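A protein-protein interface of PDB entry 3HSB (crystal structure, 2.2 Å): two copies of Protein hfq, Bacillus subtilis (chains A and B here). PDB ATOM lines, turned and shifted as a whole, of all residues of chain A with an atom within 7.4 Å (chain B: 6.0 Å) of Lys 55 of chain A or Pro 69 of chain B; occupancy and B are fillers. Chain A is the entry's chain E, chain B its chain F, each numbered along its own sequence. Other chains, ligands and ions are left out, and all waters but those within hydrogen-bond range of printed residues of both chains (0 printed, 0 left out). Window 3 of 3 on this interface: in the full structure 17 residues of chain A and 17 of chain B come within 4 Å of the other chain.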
ATOM      1  N   LEU A  36      -5.320  15.258  17.558  1.00  0.00           N
ATOM      2  CA  LEU A  36      -4.705  16.089  16.542  1.00  0.00           C
ATOM      3  C   LEU A  36      -5.510  15.929  15.271  1.00  0.00           C
ATOM      4  O   LEU A  36      -5.783  14.826  14.876  1.00  0.00           O
ATOM      5  CB  LEU A  36      -3.340  15.468  16.212  1.00  0.00           C
ATOM      6  CG  LEU A  36      -1.961  15.884  16.671  1.00  0.00           C
ATOM      7  CD1 LEU A  36      -0.933  14.910  16.134  1.00  0.00           C
ATOM      8  CD2 LEU A  36      -1.674  17.297  16.194  1.00  0.00           C
ATOM      9  N   GLN A  39      -3.860  16.254   7.860  1.00  0.00           N
ATOM     10  CA  GLN A  39      -3.788  15.476   6.663  1.00  0.00           C
ATOM     11  C   GLN A  39      -2.546  14.638   6.677  1.00  0.00           C
ATOM     12  O   GLN A  39      -1.482  15.122   7.092  1.00  0.00           O
ATOM     13  CB  GLN A  39      -3.611  16.397   5.452  1.00  0.00           C
ATOM     14  CG  GLN A  39      -4.818  17.223   5.084  1.00  0.00           C
ATOM     15  CD  GLN A  39      -4.679  17.695   3.610  1.00  0.00           C
ATOM     16  OE1 GLN A  39      -3.562  17.771   3.086  1.00  0.00           O
ATOM     17  NE2 GLN A  39      -5.810  17.955   2.939  1.00  0.00           N
ATOM     18  N   LYS A  41       0.557  13.038   5.107  1.00  0.00           N
ATOM     19  CA  LYS A  41       1.474  13.267   4.017  1.00  0.00           C
ATOM     20  C   LYS A  41       2.199  12.014   3.617  1.00  0.00           C
ATOM     21  O   LYS A  41       2.664  11.912   2.507  1.00  0.00           O
ATOM     22  CB  LYS A  41       2.438  14.343   4.395  1.00  0.00           C
ATOM     23  CG  LYS A  41       1.740  15.701   4.723  1.00  0.00           C
ATOM     24  CD  LYS A  41       1.407  16.555   3.473  1.00  0.00           C
ATOM     25  CE  LYS A  41      -0.029  16.389   3.025  1.00  0.00           C
ATOM     26  NZ  LYS A  41      -0.640  17.678   2.418  1.00  0.00           N
ATOM     27  N   LEU A  49       3.474  10.522   8.940  1.00  0.00           N
ATOM     28  CA  LEU A  49       3.708  11.984   8.760  1.00  0.00           C
ATOM     29  C   LEU A  49       2.400  12.717   8.512  1.00  0.00           C
ATOM     30  O   LEU A  49       1.747  12.506   7.520  1.00  0.00           O
ATOM     31  CB  LEU A  49       4.664  12.280   7.599  1.00  0.00           C
ATOM     32  CG  LEU A  49       5.160  13.738   7.455  1.00  0.00           C
ATOM     33  CD1 LEU A  49       5.923  14.238   8.716  1.00  0.00           C
ATOM     34  CD2 LEU A  49       6.060  13.761   6.264  1.00  0.00           C
ATOM     35  N   LEU A  50       2.021  13.560   9.462  1.00  0.00           N
ATOM     36  CA  LEU A  50       0.805  14.299   9.427  1.00  0.00           C
ATOM     37  C   LEU A  50       1.166  15.823   9.229  1.00  0.00           C
ATOM     38  O   LEU A  50       2.255  16.284   9.592  1.00  0.00           O
ATOM     39  CB  LEU A  50       0.030  14.071  10.748  1.00  0.00           C
ATOM     40  CG  LEU A  50      -1.417  14.540  10.836  1.00  0.00           C
ATOM     41  CD1 LEU A  50      -2.393  13.570  10.181  1.00  0.00           C
ATOM     42  CD2 LEU A  50      -1.809  14.768  12.230  1.00  0.00           C
ATOM     43  N   GLU A  51       0.271  16.593   8.635  1.00  0.00           N
ATOM     44  CA  GLU A  51       0.405  18.064   8.649  1.00  0.00           C
ATOM     45  C   GLU A  51      -0.830  18.653   9.302  1.00  0.00           C
ATOM     46  O   GLU A  51      -1.952  18.320   8.906  1.00  0.00           O
ATOM     47  CB  GLU A  51       0.551  18.577   7.226  1.00  0.00           C
ATOM     48  CG  GLU A  51       1.183  19.968   7.114  1.00  0.00           C
ATOM     49  CD  GLU A  51       1.258  20.416   5.673  1.00  0.00           C
ATOM     50  OE1 GLU A  51       2.351  20.235   5.074  1.00  0.00           O
ATOM     51  OE2 GLU A  51       0.216  20.859   5.122  1.00  0.00           O
ATOM     52  N   SER A  52      -0.641  19.452  10.353  1.00  0.00           N
ATOM     53  CA  SER A  52      -1.705  20.089  11.127  1.00  0.00           C
ATOM     54  C   SER A  52      -1.366  21.577  11.031  1.00  0.00           C
ATOM     55  O   SER A  52      -0.297  22.040  11.476  1.00  0.00           O
ATOM     56  CB  SER A  52      -1.623  19.654  12.605  1.00  0.00           C
ATOM     57  OG  SER A  52      -2.882  19.312  13.239  1.00  0.00           O
ATOM     58  N   GLU A  53      -2.291  22.315  10.413  1.00  0.00           N
ATOM     59  CA  GLU A  53      -2.127  23.743  10.036  1.00  0.00           C
ATOM     60  C   GLU A  53      -0.762  24.139   9.487  1.00  0.00           C
ATOM     61  O   GLU A  53      -0.073  25.007  10.068  1.00  0.00           O
ATOM     62  CB  GLU A  53      -2.482  24.629  11.199  1.00  0.00           C
ATOM     63  CG  GLU A  53      -2.107  24.025  12.500  1.00  0.00           C
ATOM     64  CD  GLU A  53      -3.133  24.322  13.547  1.00  0.00           C
ATOM     65  OE1 GLU A  53      -4.335  24.515  13.157  1.00  0.00           O
ATOM     66  OE2 GLU A  53      -2.722  24.366  14.738  1.00  0.00           O
ATOM     67  N   GLY A  54      -0.356  23.509   8.385  1.00  0.00           N
ATOM     68  CA  GLY A  54       0.944  23.825   7.815  1.00  0.00           C
ATOM     69  C   GLY A  54       2.184  23.270   8.519  1.00  0.00           C
ATOM     70  O   GLY A  54       3.271  23.342   7.931  1.00  0.00           O
ATOM     71  N   LYS A  55       2.036  22.712   9.736  1.00  0.00           N
ATOM     72  CA  LYS A  55       3.178  22.111  10.436  1.00  0.00           C
ATOM     73  C   LYS A  55       3.279  20.560  10.319  1.00  0.00           C
ATOM     74  O   LYS A  55       2.352  19.848  10.589  1.00  0.00           O
ATOM     75  CB  LYS A  55       3.295  22.562  11.922  1.00  0.00           C
ATOM     76  CG  LYS A  55       4.663  21.932  12.635  1.00  0.00           C
ATOM     77  CD  LYS A  55       4.828  21.939  14.187  1.00  0.00           C
ATOM     78  CE  LYS A  55       3.517  21.611  14.981  1.00  0.00           C
ATOM     79  NZ  LYS A  55       2.681  22.856  15.285  1.00  0.00           N
ATOM     80  N   GLN A  56       4.433  20.060   9.926  1.00  0.00           N
ATOM     81  CA  GLN A  56       4.703  18.643  10.022  1.00  0.00           C
ATOM     82  C   GLN A  56       4.662  18.108  11.442  1.00  0.00           C
ATOM     83  O   GLN A  56       5.114  18.756  12.424  1.00  0.00           O
ATOM     84  CB  GLN A  56       6.049  18.305   9.406  1.00  0.00           C
ATOM     85  CG  GLN A  56       6.037  18.482   7.934  1.00  0.00           C
ATOM     86  CD  GLN A  56       7.331  18.133   7.332  1.00  0.00           C
ATOM     87  OE1 GLN A  56       8.363  18.086   8.004  1.00  0.00           O
ATOM     88  NE2 GLN A  56       7.326  17.942   6.037  1.00  0.00           N
ATOM     89  N   GLN A  57       4.058  16.937  11.587  1.00  0.00           N
ATOM     90  CA  GLN A  57       4.332  16.165  12.800  1.00  0.00           C
ATOM     91  C   GLN A  57       4.648  14.711  12.422  1.00  0.00           C
ATOM     92  O   GLN A  57       3.839  14.107  11.799  1.00  0.00           O
ATOM     93  CB  GLN A  57       3.163  16.255  13.747  1.00  0.00           C
ATOM     94  CG  GLN A  57       3.174  17.551  14.531  1.00  0.00           C
ATOM     95  CD  GLN A  57       2.310  17.536  15.744  1.00  0.00           C
ATOM     96  OE1 GLN A  57       1.302  18.227  15.782  1.00  0.00           O
ATOM     97  NE2 GLN A  57       2.666  16.730  16.744  1.00  0.00           N
ATOM     98  N   LEU A  58       5.794  14.178  12.825  1.00  0.00           N
ATOM     99  CA  LEU A  58       6.081  12.757  12.668  1.00  0.00           C
ATOM    100  C   LEU A  58       5.576  12.056  13.939  1.00  0.00           C
ATOM    101  O   LEU A  58       6.087  12.301  15.038  1.00  0.00           O
ATOM    102  CB  LEU A  58       7.577  12.508  12.499  1.00  0.00           C
ATOM    103  CG  LEU A  58       7.868  11.071  12.025  1.00  0.00           C
ATOM    104  CD1 LEU A  58       7.376  10.769  10.574  1.00  0.00           C
ATOM    105  CD2 LEU A  58       9.341  10.685  12.172  1.00  0.00           C
ATOM    106  N   PHE B  15      13.226  11.798   7.835  1.00  0.00           N
ATOM    107  CA  PHE B  15      12.848  12.877   8.755  1.00  0.00           C
ATOM    108  C   PHE B  15      13.915  13.114   9.791  1.00  0.00           C
ATOM    109  O   PHE B  15      14.435  14.254   9.914  1.00  0.00           O
ATOM    110  CB  PHE B  15      11.472  12.577   9.370  1.00  0.00           C
ATOM    111  CG  PHE B  15      10.967  13.642  10.309  1.00  0.00           C
ATOM    112  CD1 PHE B  15      10.061  14.582   9.861  1.00  0.00           C
ATOM    113  CD2 PHE B  15      11.397  13.686  11.675  1.00  0.00           C
ATOM    114  CE1 PHE B  15       9.574  15.599  10.717  1.00  0.00           C
ATOM    115  CE2 PHE B  15      10.872  14.653  12.591  1.00  0.00           C
ATOM    116  CZ  PHE B  15       9.928  15.607  12.086  1.00  0.00           C
ATOM    117  N   ILE B  19      16.448  16.445  10.162  1.00  0.00           N
ATOM    118  CA  ILE B  19      16.415  17.415  11.244  1.00  0.00           C
ATOM    119  C   ILE B  19      17.753  17.333  11.936  1.00  0.00           C
ATOM    120  O   ILE B  19      18.255  18.352  12.435  1.00  0.00           O
ATOM    121  CB  ILE B  19      15.184  17.300  12.265  1.00  0.00           C
ATOM    122  CG1 ILE B  19      15.049  15.905  12.842  1.00  0.00           C
ATOM    123  CG2 ILE B  19      13.838  17.791  11.644  1.00  0.00           C
ATOM    124  CD1 ILE B  19      14.378  15.932  14.189  1.00  0.00           C
ATOM    125  N   THR B  24      17.746  21.225  13.052  1.00  0.00           N
ATOM    126  CA  THR B  24      16.422  21.783  13.294  1.00  0.00           C
ATOM    127  C   THR B  24      16.021  21.556  14.773  1.00  0.00           C
ATOM    128  O   THR B  24      16.143  20.420  15.291  1.00  0.00           O
ATOM    129  CB  THR B  24      15.384  21.077  12.423  1.00  0.00           C
ATOM    130  OG1 THR B  24      15.863  20.996  11.068  1.00  0.00           O
ATOM    131  CG2 THR B  24      14.026  21.797  12.473  1.00  0.00           C
ATOM    132  N   TYR B  25      15.517  22.598  15.446  1.00  0.00           N
ATOM    133  CA  TYR B  25      14.983  22.399  16.757  1.00  0.00           C
ATOM    134  C   TYR B  25      13.697  21.626  16.601  1.00  0.00           C
ATOM    135  O   TYR B  25      12.893  21.867  15.674  1.00  0.00           O
ATOM    136  CB  TYR B  25      14.663  23.694  17.420  1.00  0.00           C
ATOM    137  CG  TYR B  25      15.853  24.332  18.079  1.00  0.00           C
ATOM    138  CD1 TYR B  25      16.592  25.304  17.372  1.00  0.00           C
ATOM    139  CD2 TYR B  25      16.233  24.000  19.396  1.00  0.00           C
ATOM    140  CE1 TYR B  25      17.732  25.970  17.963  1.00  0.00           C
ATOM    141  CE2 TYR B  25      17.366  24.657  20.017  1.00  0.00           C
ATOM    142  CZ  TYR B  25      18.086  25.657  19.269  1.00  0.00           C
ATOM    143  OH  TYR B  25      19.190  26.344  19.783  1.00  0.00           O
ATOM    144  N   VAL B  26      13.465  20.713  17.530  1.00  0.00           N
ATOM    145  CA  VAL B  26      12.277  19.932  17.442  1.00  0.00           C
ATOM    146  C   VAL B  26      11.686  19.861  18.851  1.00  0.00           C
ATOM    147  O   VAL B  26      12.441  19.743  19.877  1.00  0.00           O
ATOM    148  CB  VAL B  26      12.689  18.557  16.807  1.00  0.00           C
ATOM    149  CG1 VAL B  26      13.493  17.668  17.777  1.00  0.00           C
ATOM    150  CG2 VAL B  26      11.561  17.802  16.224  1.00  0.00           C
ATOM    151  N   THR B  27      10.350  19.923  18.909  1.00  0.00           N
ATOM    152  CA  THR B  27       9.634  19.539  20.102  1.00  0.00           C
ATOM    153  C   THR B  27       9.299  18.032  20.019  1.00  0.00           C
ATOM    154  O   THR B  27       8.710  17.570  19.027  1.00  0.00           O
ATOM    155  CB  THR B  27       8.305  20.365  20.257  1.00  0.00           C
ATOM    156  OG1 THR B  27       8.624  21.777  20.196  1.00  0.00           O
ATOM    157  CG2 THR B  27       7.639  20.081  21.576  1.00  0.00           C
ATOM    158  N   PHE B  67       7.243  14.086  16.987  1.00  0.00           N
ATOM    159  CA  PHE B  67       8.233  15.155  16.749  1.00  0.00           C
ATOM    160  C   PHE B  67       7.515  16.253  15.914  1.00  0.00           C
ATOM    161  O   PHE B  67       6.840  15.994  14.906  1.00  0.00           O
ATOM    162  CB  PHE B  67       9.419  14.702  15.857  1.00  0.00           C
ATOM    163  CG  PHE B  67      10.220  13.538  16.414  1.00  0.00           C
ATOM    164  CD1 PHE B  67       9.851  12.233  16.137  1.00  0.00           C
ATOM    165  CD2 PHE B  67      11.380  13.777  17.130  1.00  0.00           C
ATOM    166  CE1 PHE B  67      10.580  11.198  16.602  1.00  0.00           C
ATOM    167  CE2 PHE B  67      12.105  12.737  17.645  1.00  0.00           C
ATOM    168  CZ  PHE B  67      11.704  11.432  17.385  1.00  0.00           C
ATOM    169  N   ALA B  68       7.720  17.470  16.349  1.00  0.00           N
ATOM    170  CA  ALA B  68       7.121  18.589  15.672  1.00  0.00           C
ATOM    171  C   ALA B  68       8.303  19.502  15.389  1.00  0.00           C
ATOM    172  O   ALA B  68       8.818  20.075  16.297  1.00  0.00           O
ATOM    173  CB  ALA B  68       6.058  19.245  16.665  1.00  0.00           C
ATOM    174  N   PRO B  69       8.791  19.554  14.144  1.00  0.00           N
ATOM    175  CA  PRO B  69       9.903  20.409  13.894  1.00  0.00           C
ATOM    176  C   PRO B  69       9.514  21.864  13.914  1.00  0.00           C
ATOM    177  O   PRO B  69       8.383  22.158  13.596  1.00  0.00           O
ATOM    178  CB  PRO B  69      10.374  19.988  12.484  1.00  0.00           C
ATOM    179  CG  PRO B  69       9.329  19.201  11.908  1.00  0.00           C
ATOM    180  CD  PRO B  69       8.322  18.851  12.931  1.00  0.00           C
ATOM    181  N   GLN B  70      10.437  22.749  14.309  1.00  0.00           N
ATOM    182  CA  GLN B  70      10.342  24.201  14.068  1.00  0.00           C
ATOM    183  C   GLN B  70      10.086  24.580  12.571  1.00  0.00           C
ATOM    184  O   GLN B  70       9.244  25.424  12.258  1.00  0.00           O
ATOM    185  CB  GLN B  70      11.636  24.876  14.578  1.00  0.00           C
ATOM    186  CG  GLN B  70      11.436  26.186  15.410  1.00  0.00           C
ATOM    187  CD  GLN B  70      12.746  27.080  15.571  1.00  0.00           C
ATOM    188  OE1 GLN B  70      13.347  27.527  14.586  1.00  0.00           O
ATOM    189  NE2 GLN B  70      13.148  27.333  16.815  1.00  0.00           N
ATOM    190  N   LYS B  71      10.794  23.959  11.632  1.00  0.00           N
ATOM    191  CA  LYS B  71      10.574  24.203  10.188  1.00  0.00           C
ATOM    192  C   LYS B  71      10.335  22.877   9.532  1.00  0.00           C
ATOM    193  O   LYS B  71      10.893  21.867   9.972  1.00  0.00           O
ATOM    194  CB  LYS B  71      11.824  24.833   9.529  1.00  0.00           C
ATOM    195  CG  LYS B  71      12.507  25.953  10.368  1.00  0.00           C
ATOM    196  CD  LYS B  71      11.530  27.175  10.502  1.00  0.00           C
ATOM    197  CE  LYS B  71      11.495  27.844  11.879  1.00  0.00           C
ATOM    198  NZ  LYS B  71      10.239  28.686  11.977  1.00  0.00           N
ATOM    199  N   ASN B  72       9.551  22.864   8.451  1.00  0.00           N
ATOM    200  CA  ASN B  72       9.183  21.582   7.871  1.00  0.00           C
ATOM    201  C   ASN B  72      10.350  21.010   7.088  1.00  0.00           C
ATOM    202  O   ASN B  72      11.142  21.741   6.485  1.00  0.00           O
ATOM    203  CB  ASN B  72       7.893  21.619   7.030  1.00  0.00           C
ATOM    204  CG  ASN B  72       6.659  22.043   7.838  1.00  0.00           C
ATOM    205  OD1 ASN B  72       6.552  21.780   9.048  1.00  0.00           O
ATOM    206  ND2 ASN B  72       5.706  22.702   7.153  1.00  0.00           N
ATOM    207  N   VAL B  73      10.434  19.685   7.156  1.00  0.00           N
ATOM    208  CA  VAL B  73      11.466  18.843   6.553  1.00  0.00           C
ATOM    209  C   VAL B  73      11.002  18.565   5.097  1.00  0.00           C
ATOM    210  O   VAL B  73       9.814  18.320   4.883  1.00  0.00           O
ATOM    211  CB  VAL B  73      11.529  17.545   7.431  1.00  0.00           C
ATOM    212  CG1 VAL B  73      12.375  16.495   6.853  1.00  0.00           C
ATOM    213  CG2 VAL B  73      11.998  17.892   8.786  1.00  0.00           C
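Printed residues of chain B that touch a printed residue of chain A: Phe 15, Phe 67, Ala 68, Pro 69, Asn 72 and Val 73.
Hydrophobic or aromatic side chains of chain B within 4 Å of the printed part of chain A: Phe 15, Phe 67, Ala 68, Pro 69 and Val 73.
Along chain B the printed residues that touch a printed residue of chain A span positions 15 to 73.
Of the 13 printed residues of chain A, 5 touch a printed residue of chain B.
Printed residues of chain A that touch a printed residue of chain B: Gly 54, Lys 55, Gln 56, Gln 57 and Leu 58.
Hydrophobic or aromatic side chains of chain A that line the printed part of chain B: Leu 58.
Among the printed residues, 13 pairs touch across the chains.
Among the printed residues, no Asp or Glu carboxylate lies within 4 Å of a Lys or Arg side-chain nitrogen of the other chain.
No position is printed for both chains.
Of the 13 pairs that touch across the chains among the printed residues, none has its exchanged pair printed and touching as well.
CB of Ala 68 of chain B touches CE of Lys 55 of chain A, at 3.9 Å.
CD of Lys 55 of chain A touches O of Pro 69 of chain B (3.6 Å).
OD1 of Asn 72 of chain B touches CA of Lys 55 of chain A, at 3.7 Å.
Gln 56 of chain A touches Phe 15 of chain B.
Gln 56 of chain A touches Ala 68 of chain B (O to CA, 3.8 Å).
Gln 56 of chain A touches Pro 69 of chain B (O to CD, 3.2 Å).
CA of Gln 57 of chain A touches O of Phe 67 of chain B (3.3 Å).
Gln 57 of chain A touches Ala 68 of chain B.
Phe 15 of chain B touches Leu 58 of chain A.
The side-chain amide oxygen of Gln 56 of chain A sits at hydrogen-bond distance from the backbone NH of Val 73 of chain B (2.8 Å).
The side-chain amide nitrogen (ND2) of Asn 72 of chain B lies within hydrogen-bond range of the backbone carbonyl oxygen (O) of Gly 54 of chain A (2.6 Å).
N of Gln 56 of chain A lies within hydrogen-bond range of OD1 of Asn 72 of chain B (2.9 Å).
The backbone NH (N) of Phe 67 of chain B sits at hydrogen-bond distance from the backbone carbonyl oxygen (O) of Leu 58 of chain A, 2.9 Å away.
The backbone NH (N) of Gln 57 of chain A sits at hydrogen-bond distance from the backbone carbonyl oxygen (O) of Leu 50 of chain A (2.8 Å).
The backbone carbonyl oxygen of Thr 27 of chain B sits at hydrogen-bond distance from the backbone NH of Ala 68 of chain B, at 2.9 Å.
Printed residues of chain B within 4 Å of Gln 57 of chain A: Phe 67 and Ala 68.
Of the printed residues of chain A, Ala 68 of chain B touches Lys 55, Gln 56 and Gln 57.
Of the printed residues of chain B, Gln 56 of chain A touches Phe 15 (3.9 Å), Ala 68 (3.8 Å), Pro 69 (3.2 Å), Asn 72 (2.9 Å) and Val 73 (2.8 Å).
Printed residues of chain A within 4 Å of Phe 15 of chain B: Gln 56 (3.9 Å) and Leu 58 (3.7 Å).
The nearest residue of chain A that does not touch Pro 69 of chain B is Gln 57 of chain A (4.8 Å).
The nearest printed residue of chain B that does not touch Gly 54 of chain A is Lys 71 of chain B (7.3 Å).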
